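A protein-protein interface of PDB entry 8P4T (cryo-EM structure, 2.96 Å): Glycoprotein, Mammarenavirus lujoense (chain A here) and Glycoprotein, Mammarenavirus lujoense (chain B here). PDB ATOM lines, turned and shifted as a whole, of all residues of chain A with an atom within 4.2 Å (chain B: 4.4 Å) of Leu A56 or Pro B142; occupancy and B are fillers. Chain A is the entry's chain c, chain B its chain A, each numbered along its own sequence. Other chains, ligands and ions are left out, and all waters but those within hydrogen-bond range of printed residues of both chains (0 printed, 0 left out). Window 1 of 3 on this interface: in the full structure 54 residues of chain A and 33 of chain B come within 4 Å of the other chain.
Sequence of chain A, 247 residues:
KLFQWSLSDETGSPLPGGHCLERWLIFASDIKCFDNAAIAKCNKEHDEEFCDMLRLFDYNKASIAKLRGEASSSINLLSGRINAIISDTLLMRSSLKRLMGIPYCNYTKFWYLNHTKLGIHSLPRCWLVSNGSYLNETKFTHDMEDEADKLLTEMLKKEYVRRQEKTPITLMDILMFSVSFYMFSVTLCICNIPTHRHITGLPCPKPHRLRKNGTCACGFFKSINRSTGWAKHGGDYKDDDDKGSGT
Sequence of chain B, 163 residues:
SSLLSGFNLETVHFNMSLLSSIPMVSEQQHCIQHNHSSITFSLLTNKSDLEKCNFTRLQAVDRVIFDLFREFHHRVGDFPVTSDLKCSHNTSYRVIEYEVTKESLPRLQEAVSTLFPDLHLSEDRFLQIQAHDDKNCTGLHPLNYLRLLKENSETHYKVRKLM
CE of Met A53 touches CE of Met B16 (3.7 Å).
CD1 of Ile B22 touches O of Leu A56 (3.98 Å).
CB of Pro B142 touches CD2 of Leu A56, at 3.8 Å.
Phe A57 touches Leu B19.
Tyr A59 touches Ile B22 (CD2 to CD1, 3.8 Å).
Asn A60 touches Leu B19.
Asn A60 touches Ile B22.
Hydrophobic or aromatic side chains of chain B within 4 Å of the printed part of chain A: Met B16, Leu B19, Ile B22 and Pro B142.
Hydrophobic or aromatic side chains of chain A that line the printed part of chain B: Met A53, Leu A56, Phe A57 and Tyr A59.
Among the printed residues, 7 pairs touch across the chains.
Of chain B, only Ile B22 and Pro B142 come within 4 Å of Leu A56.
Printed residues of chain B within 4 Å of Tyr A59: Ile B22.
Printed residues of chain B within 4 Å of Asn A60: Leu B19 (3.5 Å) and Ile B22 (3.5 Å).
Ile A85 touches none of the printed residues of chain B.
Of the printed residues of chain A, Met B16 touches Met A53.
Printed residues of chain A within 4 Å of Ile B22: Leu A56 (3.98 Å), Tyr A59 (3.8 Å) and Asn A60 (3.5 Å).
Of chain A, only Leu A56 (3.8 Å) comes within 4 Å of Pro B142.
Leu B143 touches none of the printed residues of chain A.
The nearest printed residue of chain A that does not touch Pro B142 is Met A53 (4.9 Å).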
ATOM      1  N   ASP A  52     -30.701  16.958 -35.770  1.00  0.00           N
ATOM      2  CA  ASP A  52     -29.927  17.655 -34.748  1.00  0.00           C
ATOM      3  C   ASP A  52     -28.736  16.815 -34.302  1.00  0.00           C
ATOM      4  O   ASP A  52     -27.633  17.339 -34.100  1.00  0.00           O
ATOM      5  CB  ASP A  52     -30.818  18.009 -33.559  1.00  0.00           C
ATOM      6  CG  ASP A  52     -31.351  19.426 -33.633  1.00  0.00           C
ATOM      7  OD1 ASP A  52     -31.168  20.082 -34.681  1.00  0.00           O
ATOM      8  OD2 ASP A  52     -31.949  19.884 -32.637  1.00  0.00           O
ATOM      9  N   MET A  53     -28.937  15.507 -34.149  1.00  0.00           N
ATOM     10  CA  MET A  53     -27.824  14.639 -33.789  1.00  0.00           C
ATOM     11  C   MET A  53     -26.816  14.553 -34.927  1.00  0.00           C
ATOM     12  O   MET A  53     -25.611  14.416 -34.680  1.00  0.00           O
ATOM     13  CB  MET A  53     -28.336  13.249 -33.411  1.00  0.00           C
ATOM     14  CG  MET A  53     -29.028  13.185 -32.058  1.00  0.00           C
ATOM     15  SD  MET A  53     -27.967  13.732 -30.705  1.00  0.00           S
ATOM     16  CE  MET A  53     -26.707  12.460 -30.722  1.00  0.00           C
ATOM     17  N   LEU A  54     -27.285  14.633 -36.176  1.00  0.00           N
ATOM     18  CA  LEU A  54     -26.356  14.709 -37.303  1.00  0.00           C
ATOM     19  C   LEU A  54     -25.508  15.979 -37.243  1.00  0.00           C
ATOM     20  O   LEU A  54     -24.299  15.939 -37.509  1.00  0.00           O
ATOM     21  CB  LEU A  54     -27.130  14.643 -38.620  1.00  0.00           C
ATOM     22  CG  LEU A  54     -27.559  13.255 -39.094  1.00  0.00           C
ATOM     23  CD1 LEU A  54     -28.335  13.350 -40.396  1.00  0.00           C
ATOM     24  CD2 LEU A  54     -26.346  12.356 -39.256  1.00  0.00           C
ATOM     25  N   ARG A  55     -26.119  17.115 -36.887  1.00  0.00           N
ATOM     26  CA  ARG A  55     -25.339  18.344 -36.710  1.00  0.00           C
ATOM     27  C   ARG A  55     -24.337  18.196 -35.575  1.00  0.00           C
ATOM     28  O   ARG A  55     -23.209  18.695 -35.661  1.00  0.00           O
ATOM     29  CB  ARG A  55     -26.229  19.563 -36.434  1.00  0.00           C
ATOM     30  CG  ARG A  55     -26.928  20.244 -37.612  1.00  0.00           C
ATOM     31  CD  ARG A  55     -28.095  19.476 -38.136  1.00  0.00           C
ATOM     32  NE  ARG A  55     -28.796  20.154 -39.217  1.00  0.00           N
ATOM     33  CZ  ARG A  55     -29.780  21.024 -39.040  1.00  0.00           C
ATOM     34  NH1 ARG A  55     -30.194  21.362 -37.830  1.00  0.00           N
ATOM     35  NH2 ARG A  55     -30.369  21.562 -40.104  1.00  0.00           N
ATOM     36  N   LEU A  56     -24.733  17.511 -34.500  1.00  0.00           N
ATOM     37  CA  LEU A  56     -23.816  17.290 -33.386  1.00  0.00           C
ATOM     38  C   LEU A  56     -22.626  16.433 -33.803  1.00  0.00           C
ATOM     39  O   LEU A  56     -21.485  16.717 -33.424  1.00  0.00           O
ATOM     40  CB  LEU A  56     -24.556  16.642 -32.217  1.00  0.00           C
ATOM     41  CG  LEU A  56     -23.917  16.799 -30.838  1.00  0.00           C
ATOM     42  CD1 LEU A  56     -23.770  18.266 -30.477  1.00  0.00           C
ATOM     43  CD2 LEU A  56     -24.735  16.066 -29.788  1.00  0.00           C
ATOM     44  N   PHE A  57     -22.869  15.383 -34.589  1.00  0.00           N
ATOM     45  CA  PHE A  57     -21.769  14.544 -35.058  1.00  0.00           C
ATOM     46  C   PHE A  57     -20.867  15.296 -36.033  1.00  0.00           C
ATOM     47  O   PHE A  57     -19.642  15.112 -36.025  1.00  0.00           O
ATOM     48  CB  PHE A  57     -22.317  13.269 -35.696  1.00  0.00           C
ATOM     49  CG  PHE A  57     -22.540  12.154 -34.717  1.00  0.00           C
ATOM     50  CD1 PHE A  57     -23.444  12.297 -33.679  1.00  0.00           C
ATOM     51  CD2 PHE A  57     -21.847  10.962 -34.835  1.00  0.00           C
ATOM     52  CE1 PHE A  57     -23.648  11.274 -32.776  1.00  0.00           C
ATOM     53  CE2 PHE A  57     -22.050   9.936 -33.934  1.00  0.00           C
ATOM     54  CZ  PHE A  57     -22.952  10.092 -32.905  1.00  0.00           C
ATOM     55  N   ASP A  58     -21.451  16.153 -36.875  1.00  0.00           N
ATOM     56  CA  ASP A  58     -20.640  16.977 -37.767  1.00  0.00           C
ATOM     57  C   ASP A  58     -19.751  17.930 -36.978  1.00  0.00           C
ATOM     58  O   ASP A  58     -18.558  18.081 -37.281  1.00  0.00           O
ATOM     59  CB  ASP A  58     -21.543  17.753 -38.724  1.00  0.00           C
ATOM     60  CG  ASP A  58     -20.814  18.219 -39.965  1.00  0.00           C
ATOM     61  OD1 ASP A  58     -20.429  17.356 -40.781  1.00  0.00           O
ATOM     62  OD2 ASP A  58     -20.625  19.442 -40.126  1.00  0.00           O
ATOM     63  N   TYR A  59     -20.313  18.578 -35.955  1.00  0.00           N
ATOM     64  CA  TYR A  59     -19.511  19.446 -35.102  1.00  0.00           C
ATOM     65  C   TYR A  59     -18.445  18.658 -34.353  1.00  0.00           C
ATOM     66  O   TYR A  59     -17.349  19.172 -34.116  1.00  0.00           O
ATOM     67  CB  TYR A  59     -20.409  20.196 -34.118  1.00  0.00           C
ATOM     68  CG  TYR A  59     -19.651  20.945 -33.044  1.00  0.00           C
ATOM     69  CD1 TYR A  59     -19.095  22.190 -33.302  1.00  0.00           C
ATOM     70  CD2 TYR A  59     -19.494  20.409 -31.773  1.00  0.00           C
ATOM     71  CE1 TYR A  59     -18.402  22.877 -32.328  1.00  0.00           C
ATOM     72  CE2 TYR A  59     -18.800  21.089 -30.793  1.00  0.00           C
ATOM     73  CZ  TYR A  59     -18.258  22.323 -31.075  1.00  0.00           C
ATOM     74  OH  TYR A  59     -17.568  23.009 -30.103  1.00  0.00           O
ATOM     75  N   ASN A  60     -18.748  17.416 -33.970  1.00  0.00           N
ATOM     76  CA  ASN A  60     -17.746  16.584 -33.312  1.00  0.00           C
ATOM     77  C   ASN A  60     -16.583  16.286 -34.246  1.00  0.00           C
ATOM     78  O   ASN A  60     -15.419  16.346 -33.836  1.00  0.00           O
ATOM     79  CB  ASN A  60     -18.377  15.281 -32.829  1.00  0.00           C
ATOM     80  CG  ASN A  60     -17.359  14.321 -32.249  1.00  0.00           C
ATOM     81  OD1 ASN A  60     -16.660  14.647 -31.290  1.00  0.00           O
ATOM     82  ND2 ASN A  60     -17.268  13.131 -32.830  1.00  0.00           N
ATOM     83  N   ILE A  85     -25.203  24.908 -33.044  1.00  0.00           N
ATOM     84  CA  ILE A  85     -25.077  23.534 -33.521  1.00  0.00           C
ATOM     85  C   ILE A  85     -26.429  22.837 -33.595  1.00  0.00           C
ATOM     86  O   ILE A  85     -26.742  22.175 -34.588  1.00  0.00           O
ATOM     87  CB  ILE A  85     -24.095  22.755 -32.621  1.00  0.00           C
ATOM     88  CG1 ILE A  85     -22.821  23.571 -32.395  1.00  0.00           C
ATOM     89  CG2 ILE A  85     -23.772  21.402 -33.229  1.00  0.00           C
ATOM     90  CD1 ILE A  85     -22.068  23.187 -31.149  1.00  0.00           C
ATOM     91  N   MET B  16     -22.308   6.927 -30.350  1.00  0.00           N
ATOM     92  CA  MET B  16     -21.822   7.908 -29.385  1.00  0.00           C
ATOM     93  C   MET B  16     -20.363   7.703 -28.995  1.00  0.00           C
ATOM     94  O   MET B  16     -19.779   8.599 -28.378  1.00  0.00           O
ATOM     95  CB  MET B  16     -22.686   7.876 -28.124  1.00  0.00           C
ATOM     96  CG  MET B  16     -24.178   7.884 -28.388  1.00  0.00           C
ATOM     97  SD  MET B  16     -24.754   9.457 -29.048  1.00  0.00           S
ATOM     98  CE  MET B  16     -26.478   9.081 -29.335  1.00  0.00           C
ATOM     99  N   LEU B  19     -18.011  10.510 -30.180  1.00  0.00           N
ATOM    100  CA  LEU B  19     -18.274  11.890 -29.770  1.00  0.00           C
ATOM    101  C   LEU B  19     -17.269  12.339 -28.704  1.00  0.00           C
ATOM    102  O   LEU B  19     -17.609  12.628 -27.558  1.00  0.00           O
ATOM    103  CB  LEU B  19     -19.706  12.019 -29.265  1.00  0.00           C
ATOM    104  CG  LEU B  19     -20.807  12.121 -30.320  1.00  0.00           C
ATOM    105  CD1 LEU B  19     -22.162  11.916 -29.677  1.00  0.00           C
ATOM    106  CD2 LEU B  19     -20.753  13.460 -31.027  1.00  0.00           C
ATOM    107  N   ILE B  22     -17.505  16.467 -27.620  1.00  0.00           N
ATOM    108  CA  ILE B  22     -18.645  16.868 -26.784  1.00  0.00           C
ATOM    109  C   ILE B  22     -18.658  16.035 -25.506  1.00  0.00           C
ATOM    110  O   ILE B  22     -18.606  14.795 -25.577  1.00  0.00           O
ATOM    111  CB  ILE B  22     -19.962  16.717 -27.553  1.00  0.00           C
ATOM    112  CG1 ILE B  22     -20.004  17.645 -28.771  1.00  0.00           C
ATOM    113  CG2 ILE B  22     -21.145  16.995 -26.639  1.00  0.00           C
ATOM    114  CD1 ILE B  22     -19.441  17.056 -30.029  1.00  0.00           C
ATOM    115  N   PRO B  23     -18.707  16.658 -24.329  1.00  0.00           N
ATOM    116  CA  PRO B  23     -18.857  15.880 -23.094  1.00  0.00           C
ATOM    117  C   PRO B  23     -20.183  15.133 -23.087  1.00  0.00           C
ATOM    118  O   PRO B  23     -21.213  15.653 -23.518  1.00  0.00           O
ATOM    119  CB  PRO B  23     -18.802  16.942 -21.989  1.00  0.00           C
ATOM    120  CG  PRO B  23     -18.229  18.160 -22.632  1.00  0.00           C
ATOM    121  CD  PRO B  23     -18.626  18.104 -24.069  1.00  0.00           C
ATOM    122  N   MET B  24     -20.148  13.905 -22.584  1.00  0.00           N
ATOM    123  CA  MET B  24     -21.324  13.054 -22.514  1.00  0.00           C
ATOM    124  C   MET B  24     -21.585  12.636 -21.073  1.00  0.00           C
ATOM    125  O   MET B  24     -20.661  12.522 -20.264  1.00  0.00           O
ATOM    126  CB  MET B  24     -21.157  11.826 -23.409  1.00  0.00           C
ATOM    127  CG  MET B  24     -21.085  12.152 -24.894  1.00  0.00           C
ATOM    128  SD  MET B  24     -20.829  10.697 -25.925  1.00  0.00           S
ATOM    129  CE  MET B  24     -19.148  10.263 -25.488  1.00  0.00           C
ATOM    130  N   HIS B 141     -24.193   9.905 -23.179  1.00  0.00           N
ATOM    131  CA  HIS B 141     -24.975  10.665 -24.140  1.00  0.00           C
ATOM    132  C   HIS B 141     -24.793  12.159 -23.909  1.00  0.00           C
ATOM    133  O   HIS B 141     -24.785  12.617 -22.760  1.00  0.00           O
ATOM    134  CB  HIS B 141     -26.461  10.300 -24.044  1.00  0.00           C
ATOM    135  CG  HIS B 141     -27.245  10.609 -25.282  1.00  0.00           C
ATOM    136  ND1 HIS B 141     -27.570  11.895 -25.656  1.00  0.00           N
ATOM    137  CD2 HIS B 141     -27.781   9.797 -26.222  1.00  0.00           C
ATOM    138  CE1 HIS B 141     -28.264  11.862 -26.779  1.00  0.00           C
ATOM    139  NE2 HIS B 141     -28.407  10.601 -27.143  1.00  0.00           N
ATOM    140  N   PRO B 142     -24.641  12.944 -24.980  1.00  0.00           N
ATOM    141  CA  PRO B 142     -24.500  14.403 -24.817  1.00  0.00           C
ATOM    142  C   PRO B 142     -25.733  15.104 -24.266  1.00  0.00           C
ATOM    143  O   PRO B 142     -25.608  16.246 -23.811  1.00  0.00           O
ATOM    144  CB  PRO B 142     -24.188  14.890 -26.241  1.00  0.00           C
ATOM    145  CG  PRO B 142     -23.747  13.681 -26.985  1.00  0.00           C
ATOM    146  CD  PRO B 142     -24.471  12.526 -26.380  1.00  0.00           C
ATOM    147  N   LEU B 143     -26.909  14.469 -24.304  1.00  0.00           N
ATOM    148  CA  LEU B 143     -28.169  15.170 -24.050  1.00  0.00           C
ATOM    149  C   LEU B 143     -28.156  15.923 -22.723  1.00  0.00           C
ATOM    150  O   LEU B 143     -28.511  17.106 -22.665  1.00  0.00           O
ATOM    151  CB  LEU B 143     -29.331  14.175 -24.083  1.00  0.00           C
ATOM    152  CG  LEU B 143     -30.687  14.706 -23.616  1.00  0.00           C
ATOM    153  CD1 LEU B 143     -31.301  15.611 -24.667  1.00  0.00           C
ATOM    154  CD2 LEU B 143     -31.627  13.563 -23.273  1.00  0.00           C
ATOM    155  N   ASN B 144     -27.765  15.246 -21.641  1.00  0.00           N
ATOM    156  CA  ASN B 144     -27.841  15.866 -20.323  1.00  0.00           C
ATOM    157  C   ASN B 144     -26.890  17.050 -20.195  1.00  0.00           C
ATOM    158  O   ASN B 144     -27.223  18.040 -19.536  1.00  0.00           O
ATOM    159  CB  ASN B 144     -27.557  14.830 -19.239  1.00  0.00           C
ATOM    160  CG  ASN B 144     -28.607  13.740 -19.189  1.00  0.00           C
ATOM    161  OD1 ASN B 144     -29.663  13.907 -18.580  1.00  0.00           O
ATOM    162  ND2 ASN B 144     -28.324  12.617 -19.839  1.00  0.00           N
ATOM    163  N   TYR B 145     -25.721  16.987 -20.836  1.00  0.00           N
ATOM    164  CA  TYR B 145     -24.791  18.108 -20.752  1.00  0.00           C
ATOM    165  C   TYR B 145     -25.304  19.307 -21.543  1.00  0.00           C
ATOM    166  O   TYR B 145     -25.122  20.458 -21.126  1.00  0.00           O
ATOM    167  CB  TYR B 145     -23.410  17.684 -21.247  1.00  0.00           C
ATOM    168  CG  TYR B 145     -22.303  18.629 -20.845  1.00  0.00           C
ATOM    169  CD1 TYR B 145     -21.671  18.504 -19.615  1.00  0.00           C
ATOM    170  CD2 TYR B 145     -21.888  19.646 -21.694  1.00  0.00           C
ATOM    171  CE1 TYR B 145     -20.659  19.365 -19.242  1.00  0.00           C
ATOM    172  CE2 TYR B 145     -20.877  20.512 -21.328  1.00  0.00           C
ATOM    173  CZ  TYR B 145     -20.266  20.366 -20.102  1.00  0.00           C
ATOM    174  OH  TYR B 145     -19.258  21.226 -19.735  1.00  0.00           O
ATOM    175  N   LEU B 146     -25.957  19.061 -22.680  1.00  0.00           N
ATOM    176  CA  LEU B 146     -26.560  20.157 -23.428  1.00  0.00           C
ATOM    177  C   LEU B 146     -27.720  20.772 -22.655  1.00  0.00           C
ATOM    178  O   LEU B 146     -27.916  21.993 -22.680  1.00  0.00           O
ATOM    179  CB  LEU B 146     -27.019  19.668 -24.801  1.00  0.00           C
ATOM    180  CG  LEU B 146     -25.975  18.914 -25.628  1.00  0.00           C
ATOM    181  CD1 LEU B 146     -26.553  18.485 -26.967  1.00  0.00           C
ATOM    182  CD2 LEU B 146     -24.727  19.760 -25.825  1.00  0.00           C
